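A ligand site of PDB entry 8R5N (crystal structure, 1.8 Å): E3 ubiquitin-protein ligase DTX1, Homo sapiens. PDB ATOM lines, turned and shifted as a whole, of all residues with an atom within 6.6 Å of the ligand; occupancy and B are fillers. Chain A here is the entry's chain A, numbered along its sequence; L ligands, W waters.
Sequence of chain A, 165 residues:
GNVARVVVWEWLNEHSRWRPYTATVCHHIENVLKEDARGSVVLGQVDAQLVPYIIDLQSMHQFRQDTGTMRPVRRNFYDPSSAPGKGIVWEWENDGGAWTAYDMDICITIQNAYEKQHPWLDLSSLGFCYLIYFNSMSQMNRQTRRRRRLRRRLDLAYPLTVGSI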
ATOM      1  N   TRP A  11     -15.692   7.732   0.174  1.00  0.00           N
ATOM      2  CA  TRP A  11     -16.726   6.695   0.047  1.00  0.00           C
ATOM      3  C   TRP A  11     -16.616   5.777   1.259  1.00  0.00           C
ATOM      4  O   TRP A  11     -15.511   5.535   1.751  1.00  0.00           O
ATOM      5  CB  TRP A  11     -16.635   5.929  -1.291  1.00  0.00           C
ATOM      6  CG  TRP A  11     -15.310   5.259  -1.521  1.00  0.00           C
ATOM      7  CD1 TRP A  11     -14.194   5.811  -2.069  1.00  0.00           C
ATOM      8  CD2 TRP A  11     -14.979   3.901  -1.224  1.00  0.00           C
ATOM      9  NE1 TRP A  11     -13.157   4.911  -2.023  1.00  0.00           N
ATOM     10  CE2 TRP A  11     -13.624   3.711  -1.546  1.00  0.00           C
ATOM     11  CE3 TRP A  11     -15.689   2.831  -0.678  1.00  0.00           C
ATOM     12  CZ2 TRP A  11     -12.960   2.513  -1.302  1.00  0.00           C
ATOM     13  CZ3 TRP A  11     -15.059   1.613  -0.563  1.00  0.00           C
ATOM     14  CH2 TRP A  11     -13.675   1.501  -0.762  1.00  0.00           C
ATOM     15  N   LEU A  12     -17.760   5.333   1.802  1.00  0.00           N
ATOM     16  CA  LEU A  12     -17.754   4.494   2.998  1.00  0.00           C
ATOM     17  C   LEU A  12     -17.561   3.003   2.661  1.00  0.00           C
ATOM     18  O   LEU A  12     -18.389   2.397   1.952  1.00  0.00           O
ATOM     19  CB  LEU A  12     -19.058   4.721   3.765  1.00  0.00           C
ATOM     20  CG  LEU A  12     -19.179   4.060   5.134  1.00  0.00           C
ATOM     21  CD1 LEU A  12     -18.274   4.695   6.152  1.00  0.00           C
ATOM     22  CD2 LEU A  12     -20.623   4.099   5.620  1.00  0.00           C
ATOM     23  N   ASN A  13     -16.469   2.419   3.162  1.00  0.00           N
ATOM     24  CA  ASN A  13     -16.181   0.993   2.911  1.00  0.00           C
ATOM     25  C   ASN A  13     -16.877   0.044   3.912  1.00  0.00           C
ATOM     26  O   ASN A  13     -17.609   0.487   4.790  1.00  0.00           O
ATOM     27  CB  ASN A  13     -14.678   0.784   2.830  1.00  0.00           C
ATOM     28  CG  ASN A  13     -13.913   0.755   4.118  1.00  0.00           C
ATOM     29  OD1 ASN A  13     -14.455   0.777   5.231  1.00  0.00           O
ATOM     30  ND2 ASN A  13     -12.604   0.644   3.973  1.00  0.00           N
ATOM     31  N   GLU A  14     -16.709  -1.287   3.705  1.00  0.00           N
ATOM     32  CA  GLU A  14     -17.268  -2.366   4.511  1.00  0.00           C
ATOM     33  C   GLU A  14     -16.821  -2.379   5.954  1.00  0.00           C
ATOM     34  O   GLU A  14     -17.503  -2.985   6.786  1.00  0.00           O
ATOM     35  CB  GLU A  14     -16.985  -3.741   3.854  1.00  0.00           C
ATOM     36  CG  GLU A  14     -15.517  -4.086   3.645  1.00  0.00           C
ATOM     37  CD  GLU A  14     -14.949  -3.680   2.306  1.00  0.00           C
ATOM     38  OE1 GLU A  14     -15.318  -2.587   1.804  1.00  0.00           O
ATOM     39  OE2 GLU A  14     -14.116  -4.429   1.758  1.00  0.00           O
ATOM     40  N   ARG A  19     -13.121   6.320   2.871  1.00  0.00           N
ATOM     41  CA  ARG A  19     -11.915   6.190   2.066  1.00  0.00           C
ATOM     42  C   ARG A  19     -11.824   7.291   1.065  1.00  0.00           C
ATOM     43  O   ARG A  19     -12.822   7.568   0.414  1.00  0.00           O
ATOM     44  CB  ARG A  19     -11.920   4.851   1.320  1.00  0.00           C
ATOM     45  CG  ARG A  19     -11.832   3.599   2.210  1.00  0.00           C
ATOM     46  CD  ARG A  19     -10.499   3.405   2.866  1.00  0.00           C
ATOM     47  NE  ARG A  19      -9.453   3.275   1.849  1.00  0.00           N
ATOM     48  CZ  ARG A  19      -8.245   3.820   1.868  1.00  0.00           C
ATOM     49  NH1 ARG A  19      -7.849   4.563   2.903  1.00  0.00           N
ATOM     50  NH2 ARG A  19      -7.421   3.655   0.843  1.00  0.00           N
ATOM     51  N   PRO A  20     -10.632   7.886   0.828  1.00  0.00           N
ATOM     52  CA  PRO A  20     -10.566   8.947  -0.164  1.00  0.00           C
ATOM     53  C   PRO A  20     -10.453   8.415  -1.586  1.00  0.00           C
ATOM     54  O   PRO A  20      -9.718   7.482  -1.838  1.00  0.00           O
ATOM     55  CB  PRO A  20      -9.308   9.708   0.238  1.00  0.00           C
ATOM     56  CG  PRO A  20      -8.400   8.644   0.802  1.00  0.00           C
ATOM     57  CD  PRO A  20      -9.304   7.658   1.472  1.00  0.00           C
ATOM     58  N   TYR A  21     -11.149   9.042  -2.528  1.00  0.00           N
ATOM     59  CA  TYR A  21     -10.904   8.850  -3.935  1.00  0.00           C
ATOM     60  C   TYR A  21      -9.570   9.589  -4.179  1.00  0.00           C
ATOM     61  O   TYR A  21      -9.165  10.436  -3.346  1.00  0.00           O
ATOM     62  CB  TYR A  21     -12.010   9.487  -4.823  1.00  0.00           C
ATOM     63  CG  TYR A  21     -13.355   8.807  -4.768  1.00  0.00           C
ATOM     64  CD1 TYR A  21     -13.620   7.685  -5.534  1.00  0.00           C
ATOM     65  CD2 TYR A  21     -14.361   9.290  -3.964  1.00  0.00           C
ATOM     66  CE1 TYR A  21     -14.871   7.079  -5.510  1.00  0.00           C
ATOM     67  CE2 TYR A  21     -15.612   8.711  -3.935  1.00  0.00           C
ATOM     68  CZ  TYR A  21     -15.856   7.582  -4.693  1.00  0.00           C
ATOM     69  OH  TYR A  21     -17.111   7.033  -4.705  1.00  0.00           O
ATOM     70  N   LEU A  43     -17.180   7.361 -13.148  1.00  0.00           N
ATOM     71  CA  LEU A  43     -15.792   7.303 -12.696  1.00  0.00           C
ATOM     72  C   LEU A  43     -14.841   6.634 -13.705  1.00  0.00           C
ATOM     73  O   LEU A  43     -13.671   7.001 -13.738  1.00  0.00           O
ATOM     74  CB  LEU A  43     -15.728   6.658 -11.305  1.00  0.00           C
ATOM     75  CG  LEU A  43     -16.517   7.371 -10.159  1.00  0.00           C
ATOM     76  CD1 LEU A  43     -16.462   6.554  -8.848  1.00  0.00           C
ATOM     77  CD2 LEU A  43     -16.018   8.767  -9.938  1.00  0.00           C
ATOM     78  N   LEU A  50     -12.150   2.082 -12.074  1.00  0.00           N
ATOM     79  CA  LEU A  50     -13.412   2.407 -11.432  1.00  0.00           C
ATOM     80  C   LEU A  50     -14.579   2.394 -12.433  1.00  0.00           C
ATOM     81  O   LEU A  50     -15.649   2.886 -12.093  1.00  0.00           O
ATOM     82  CB  LEU A  50     -13.339   3.781 -10.737  1.00  0.00           C
ATOM     83  CG  LEU A  50     -12.188   4.012  -9.746  1.00  0.00           C
ATOM     84  CD1 LEU A  50     -12.217   5.428  -9.253  1.00  0.00           C
ATOM     85  CD2 LEU A  50     -12.264   3.040  -8.550  1.00  0.00           C
ATOM     86  N   PRO A  52     -16.809   0.110 -13.012  1.00  0.00           N
ATOM     87  CA  PRO A  52     -18.121  -0.324 -12.482  1.00  0.00           C
ATOM     88  C   PRO A  52     -18.902   0.744 -11.745  1.00  0.00           C
ATOM     89  O   PRO A  52     -20.075   0.511 -11.478  1.00  0.00           O
ATOM     90  CB  PRO A  52     -17.765  -1.436 -11.482  1.00  0.00           C
ATOM     91  CG  PRO A  52     -16.362  -1.814 -11.753  1.00  0.00           C
ATOM     92  CD  PRO A  52     -15.706  -0.597 -12.322  1.00  0.00           C
ATOM     93  N   TYR A  53     -18.267   1.851 -11.315  1.00  0.00           N
ATOM     94  CA  TYR A  53     -18.900   2.780 -10.396  1.00  0.00           C
ATOM     95  C   TYR A  53     -19.370   4.104 -10.950  1.00  0.00           C
ATOM     96  O   TYR A  53     -18.662   4.751 -11.731  1.00  0.00           O
ATOM     97  CB  TYR A  53     -17.934   3.057  -9.235  1.00  0.00           C
ATOM     98  CG  TYR A  53     -17.401   1.811  -8.551  1.00  0.00           C
ATOM     99  CD1 TYR A  53     -18.215   1.045  -7.735  1.00  0.00           C
ATOM    100  CD2 TYR A  53     -16.072   1.439  -8.678  1.00  0.00           C
ATOM    101  CE1 TYR A  53     -17.717  -0.057  -7.053  1.00  0.00           C
ATOM    102  CE2 TYR A  53     -15.585   0.313  -8.029  1.00  0.00           C
ATOM    103  CZ  TYR A  53     -16.406  -0.418  -7.211  1.00  0.00           C
ATOM    104  OH  TYR A  53     -15.914  -1.538  -6.585  1.00  0.00           O
ATOM    105  N   GLN A  62     -22.424   6.165  -4.187  1.00  0.00           N
ATOM    106  CA  GLN A  62     -21.712   5.496  -5.242  1.00  0.00           C
ATOM    107  C   GLN A  62     -22.510   4.198  -5.463  1.00  0.00           C
ATOM    108  O   GLN A  62     -22.896   3.546  -4.490  1.00  0.00           O
ATOM    109  CB  GLN A  62     -20.303   5.123  -4.799  1.00  0.00           C
ATOM    110  CG  GLN A  62     -19.467   4.458  -5.884  1.00  0.00           C
ATOM    111  CD  GLN A  62     -18.206   3.838  -5.315  1.00  0.00           C
ATOM    112  OE1 GLN A  62     -17.123   4.428  -5.358  1.00  0.00           O
ATOM    113  NE2 GLN A  62     -18.311   2.616  -4.799  1.00  0.00           N
ATOM    114  N   ARG A  64     -22.621   0.446  -7.905  1.00  0.00           N
ATOM    115  CA  ARG A  64     -21.969  -0.459  -8.828  1.00  0.00           C
ATOM    116  C   ARG A  64     -23.021  -0.756  -9.907  1.00  0.00           C
ATOM    117  O   ARG A  64     -24.145  -1.113  -9.588  1.00  0.00           O
ATOM    118  CB  ARG A  64     -21.543  -1.746  -8.105  1.00  0.00           C
ATOM    119  CG  ARG A  64     -20.188  -2.279  -8.552  1.00  0.00           C
ATOM    120  CD  ARG A  64     -19.931  -3.728  -8.207  1.00  0.00           C
ATOM    121  NE  ARG A  64     -18.777  -4.202  -8.956  1.00  0.00           N
ATOM    122  CZ  ARG A  64     -18.460  -5.475  -9.170  1.00  0.00           C
ATOM    123  NH1 ARG A  64     -19.221  -6.446  -8.698  1.00  0.00           N
ATOM    124  NH2 ARG A  64     -17.383  -5.778  -9.886  1.00  0.00           N
ATOM    125  N   THR A  67     -24.336  -4.590 -10.164  1.00  0.00           N
ATOM    126  CA  THR A  67     -24.997  -5.185  -8.982  1.00  0.00           C
ATOM    127  C   THR A  67     -26.069  -4.323  -8.321  1.00  0.00           C
ATOM    128  O   THR A  67     -26.925  -4.851  -7.626  1.00  0.00           O
ATOM    129  CB  THR A  67     -23.954  -5.548  -7.920  1.00  0.00           C
ATOM    130  OG1 THR A  67     -23.399  -4.351  -7.376  1.00  0.00           O
ATOM    131  CG2 THR A  67     -22.823  -6.403  -8.458  1.00  0.00           C
ATOM    132  N   GLY A  68     -25.975  -2.999  -8.472  1.00  0.00           N
ATOM    133  CA  GLY A  68     -26.878  -2.061  -7.836  1.00  0.00           C
ATOM    134  C   GLY A  68     -26.532  -1.777  -6.386  1.00  0.00           C
ATOM    135  O   GLY A  68     -27.308  -1.095  -5.705  1.00  0.00           O
ATOM    136  N   THR A  69     -25.395  -2.288  -5.878  1.00  0.00           N
ATOM    137  CA  THR A  69     -25.007  -2.083  -4.491  1.00  0.00           C
ATOM    138  C   THR A  69     -24.584  -0.627  -4.336  1.00  0.00           C
ATOM    139  O   THR A  69     -23.959  -0.067  -5.238  1.00  0.00           O
ATOM    140  CB  THR A  69     -23.944  -3.066  -4.055  1.00  0.00           C
ATOM    141  OG1 THR A  69     -22.844  -3.001  -4.955  1.00  0.00           O
ATOM    142  CG2 THR A  69     -24.459  -4.513  -3.980  1.00  0.00           C
ATOM    143  N   MET A  70     -24.973  -0.023  -3.220  1.00  0.00           N
ATOM    144  CA  MET A  70     -24.707   1.383  -2.948  1.00  0.00           C
ATOM    145  C   MET A  70     -23.798   1.569  -1.736  1.00  0.00           C
ATOM    146  O   MET A  70     -23.876   0.808  -0.774  1.00  0.00           O
ATOM    147  CB  MET A  70     -26.028   2.125  -2.681  1.00  0.00           C
ATOM    148  CG  MET A  70     -27.044   1.980  -3.790  1.00  0.00           C
ATOM    149  SD  MET A  70     -28.461   3.073  -3.602  1.00  0.00           S
ATOM    150  CE  MET A  70     -29.242   2.366  -2.161  1.00  0.00           C
ATOM    151  N   ARG A  71     -22.977   2.611  -1.788  1.00  0.00           N
ATOM    152  CA  ARG A  71     -22.099   3.007  -0.693  1.00  0.00           C
ATOM    153  C   ARG A  71     -22.238   4.509  -0.546  1.00  0.00           C
ATOM    154  O   ARG A  71     -22.090   5.212  -1.537  1.00  0.00           O
ATOM    155  CB  ARG A  71     -20.646   2.669  -0.975  1.00  0.00           C
ATOM    156  CG  ARG A  71     -20.426   1.162  -1.082  1.00  0.00           C
ATOM    157  CD  ARG A  71     -18.964   0.810  -1.107  1.00  0.00           C
ATOM    158  NE  ARG A  71     -18.786  -0.652  -1.115  1.00  0.00           N
ATOM    159  CZ  ARG A  71     -18.872  -1.447  -0.050  1.00  0.00           C
ATOM    160  NH1 ARG A  71     -19.109  -0.943   1.159  1.00  0.00           N
ATOM    161  NH2 ARG A  71     -18.711  -2.749  -0.186  1.00  0.00           N
HETATM  162  P1  LIG L   1     -19.758  -7.862  -3.142  1.00  0.00           P
HETATM  163  O1  LIG L   1     -21.039  -7.878  -2.347  1.00  0.00           O
HETATM  164  O2  LIG L   1     -19.789  -8.798  -4.338  1.00  0.00           O
HETATM  165  O3  LIG L   1     -18.517  -8.048  -2.286  1.00  0.00           O
HETATM  166  P2  LIG L   1     -20.469  -5.067  -3.635  1.00  0.00           P
HETATM  167  O4  LIG L   1     -21.785  -5.249  -4.318  1.00  0.00           O
HETATM  168  O5  LIG L   1     -20.422  -4.636  -2.217  1.00  0.00           O
HETATM  169  O6  LIG L   1     -19.610  -6.402  -3.763  1.00  0.00           O
HETATM  170  P3  LIG L   1     -18.406  -3.033  -4.279  1.00  0.00           P
HETATM  171  O7  LIG L   1     -18.961  -1.814  -3.651  1.00  0.00           O
HETATM  172  O8  LIG L   1     -17.625  -2.925  -5.536  1.00  0.00           O
HETATM  173  O9  LIG L   1     -19.599  -4.067  -4.529  1.00  0.00           O
HETATM  174  O10 LIG L   1     -17.481  -3.732  -3.184  1.00  0.00           O
HETATM  175  C1  LIG L   1     -16.475  -4.710  -3.559  1.00  0.00           C
HETATM  176  C2  LIG L   1     -15.112  -4.212  -3.122  1.00  0.00           C
HETATM  177  O11 LIG L   1     -14.790  -2.996  -3.822  1.00  0.00           O
HETATM  178  C3  LIG L   1     -14.993  -3.888  -1.622  1.00  0.00           C
HETATM  179  O12 LIG L   1     -13.792  -4.388  -1.045  1.00  0.00           O
HETATM  180  C4  LIG L   1     -15.061  -2.359  -1.601  1.00  0.00           C
HETATM  181  O13 LIG L   1     -14.422  -1.802  -0.455  1.00  0.00           O
HETATM  182  C5  LIG L   1     -14.336  -2.012  -2.905  1.00  0.00           C
HETATM  183  N1  LIG L   1     -14.621  -0.685  -3.441  1.00  0.00           N
HETATM  184  C6  LIG L   1     -15.854  -0.099  -3.574  1.00  0.00           C
HETATM  185  N2  LIG L   1     -15.828   1.102  -4.106  1.00  0.00           N
HETATM  186  C7  LIG L   1     -14.479   1.327  -4.337  1.00  0.00           C
HETATM  187  C8  LIG L   1     -13.778   2.454  -4.805  1.00  0.00           C
HETATM  188  N3  LIG L   1     -14.376   3.609  -5.151  1.00  0.00           N
HETATM  189  N4  LIG L   1     -12.429   2.390  -4.853  1.00  0.00           N
HETATM  190  C9  LIG L   1     -11.832   1.265  -4.441  1.00  0.00           C
HETATM  191  N5  LIG L   1     -12.383   0.141  -3.960  1.00  0.00           N
HETATM  192  C10 LIG L   1     -13.721   0.239  -3.938  1.00  0.00           C
HETATM  193  O   HOH W   1     -10.703   4.480  -5.147  1.00  0.00           O
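The side-chain hydroxyl of Tyr 53 lies within hydrogen-bond range of an oxygen (O8) of the ligand (2.4 Å). An oxygen (O13) of the ligand lies within hydrogen-bond range of the side-chain carboxylate (OE1) of Glu 14 (2.6 Å). The side-chain hydroxyl of Thr 69 lies within hydrogen-bond range of an oxygen (O4) of the ligand. The guanidinium group (NE) of Arg 71 lies within salt-bridge range of an oxygen (O7) of the ligand (2.8 Å). The side-chain amide oxygen (OE1) of Gln 62 is in hydrogen-bond range of a nitrogen (N3) of the ligand. An oxygen (O8) of the ligand is in salt-bridge range of the guanidinium group (NE) of Arg 64.
N of Leu 43 is in hydrogen-bond range of O of Tyr 53 (3.3 Å). The side-chain carboxylate (OE1) of Glu 14 lies within salt-bridge range of the guanidinium group (NH2) of Arg 71. OG1 of Thr 69 sits at hydrogen-bond distance from OG1 of Thr 67 (2.8 Å). O of Thr 69 sits at hydrogen-bond distance from N of Arg 64 (3.0 Å). The backbone NH (N) of Gln 62 lies within hydrogen-bond range of the backbone carbonyl oxygen (O) of Arg 71 (2.8 Å). OE1 of Gln 62 is in hydrogen-bond range of OH of Tyr 21 (2.7 Å). The backbone carbonyl oxygen (O) of Trp 11 is in hydrogen-bond range of the backbone NH (N) of Arg 19 (2.8 Å).
Trp 11 touches the ligand (CH2 to O13, 3.4 Å). Tyr 21 touches the ligand (CE1 to N3, 3.5 Å). Leu 50 touches the ligand. Thr 67 touches the ligand. Hydrophobic or aromatic side chains that line the ligand: Trp 11, Tyr 21, Leu 50 and Tyr 53. Ten residues have an atom within 4 Å of the ligand: Trp 11, Glu 14, Tyr 21, Leu 50, Tyr 53, Gln 62, Arg 64, Thr 67, Thr 69 and Arg 71. Along chain A the residues within 4 Å of the ligand span positions 11 to 71. The nearest printed residue that does not touch the ligand is Asn 13 (4.2 Å).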
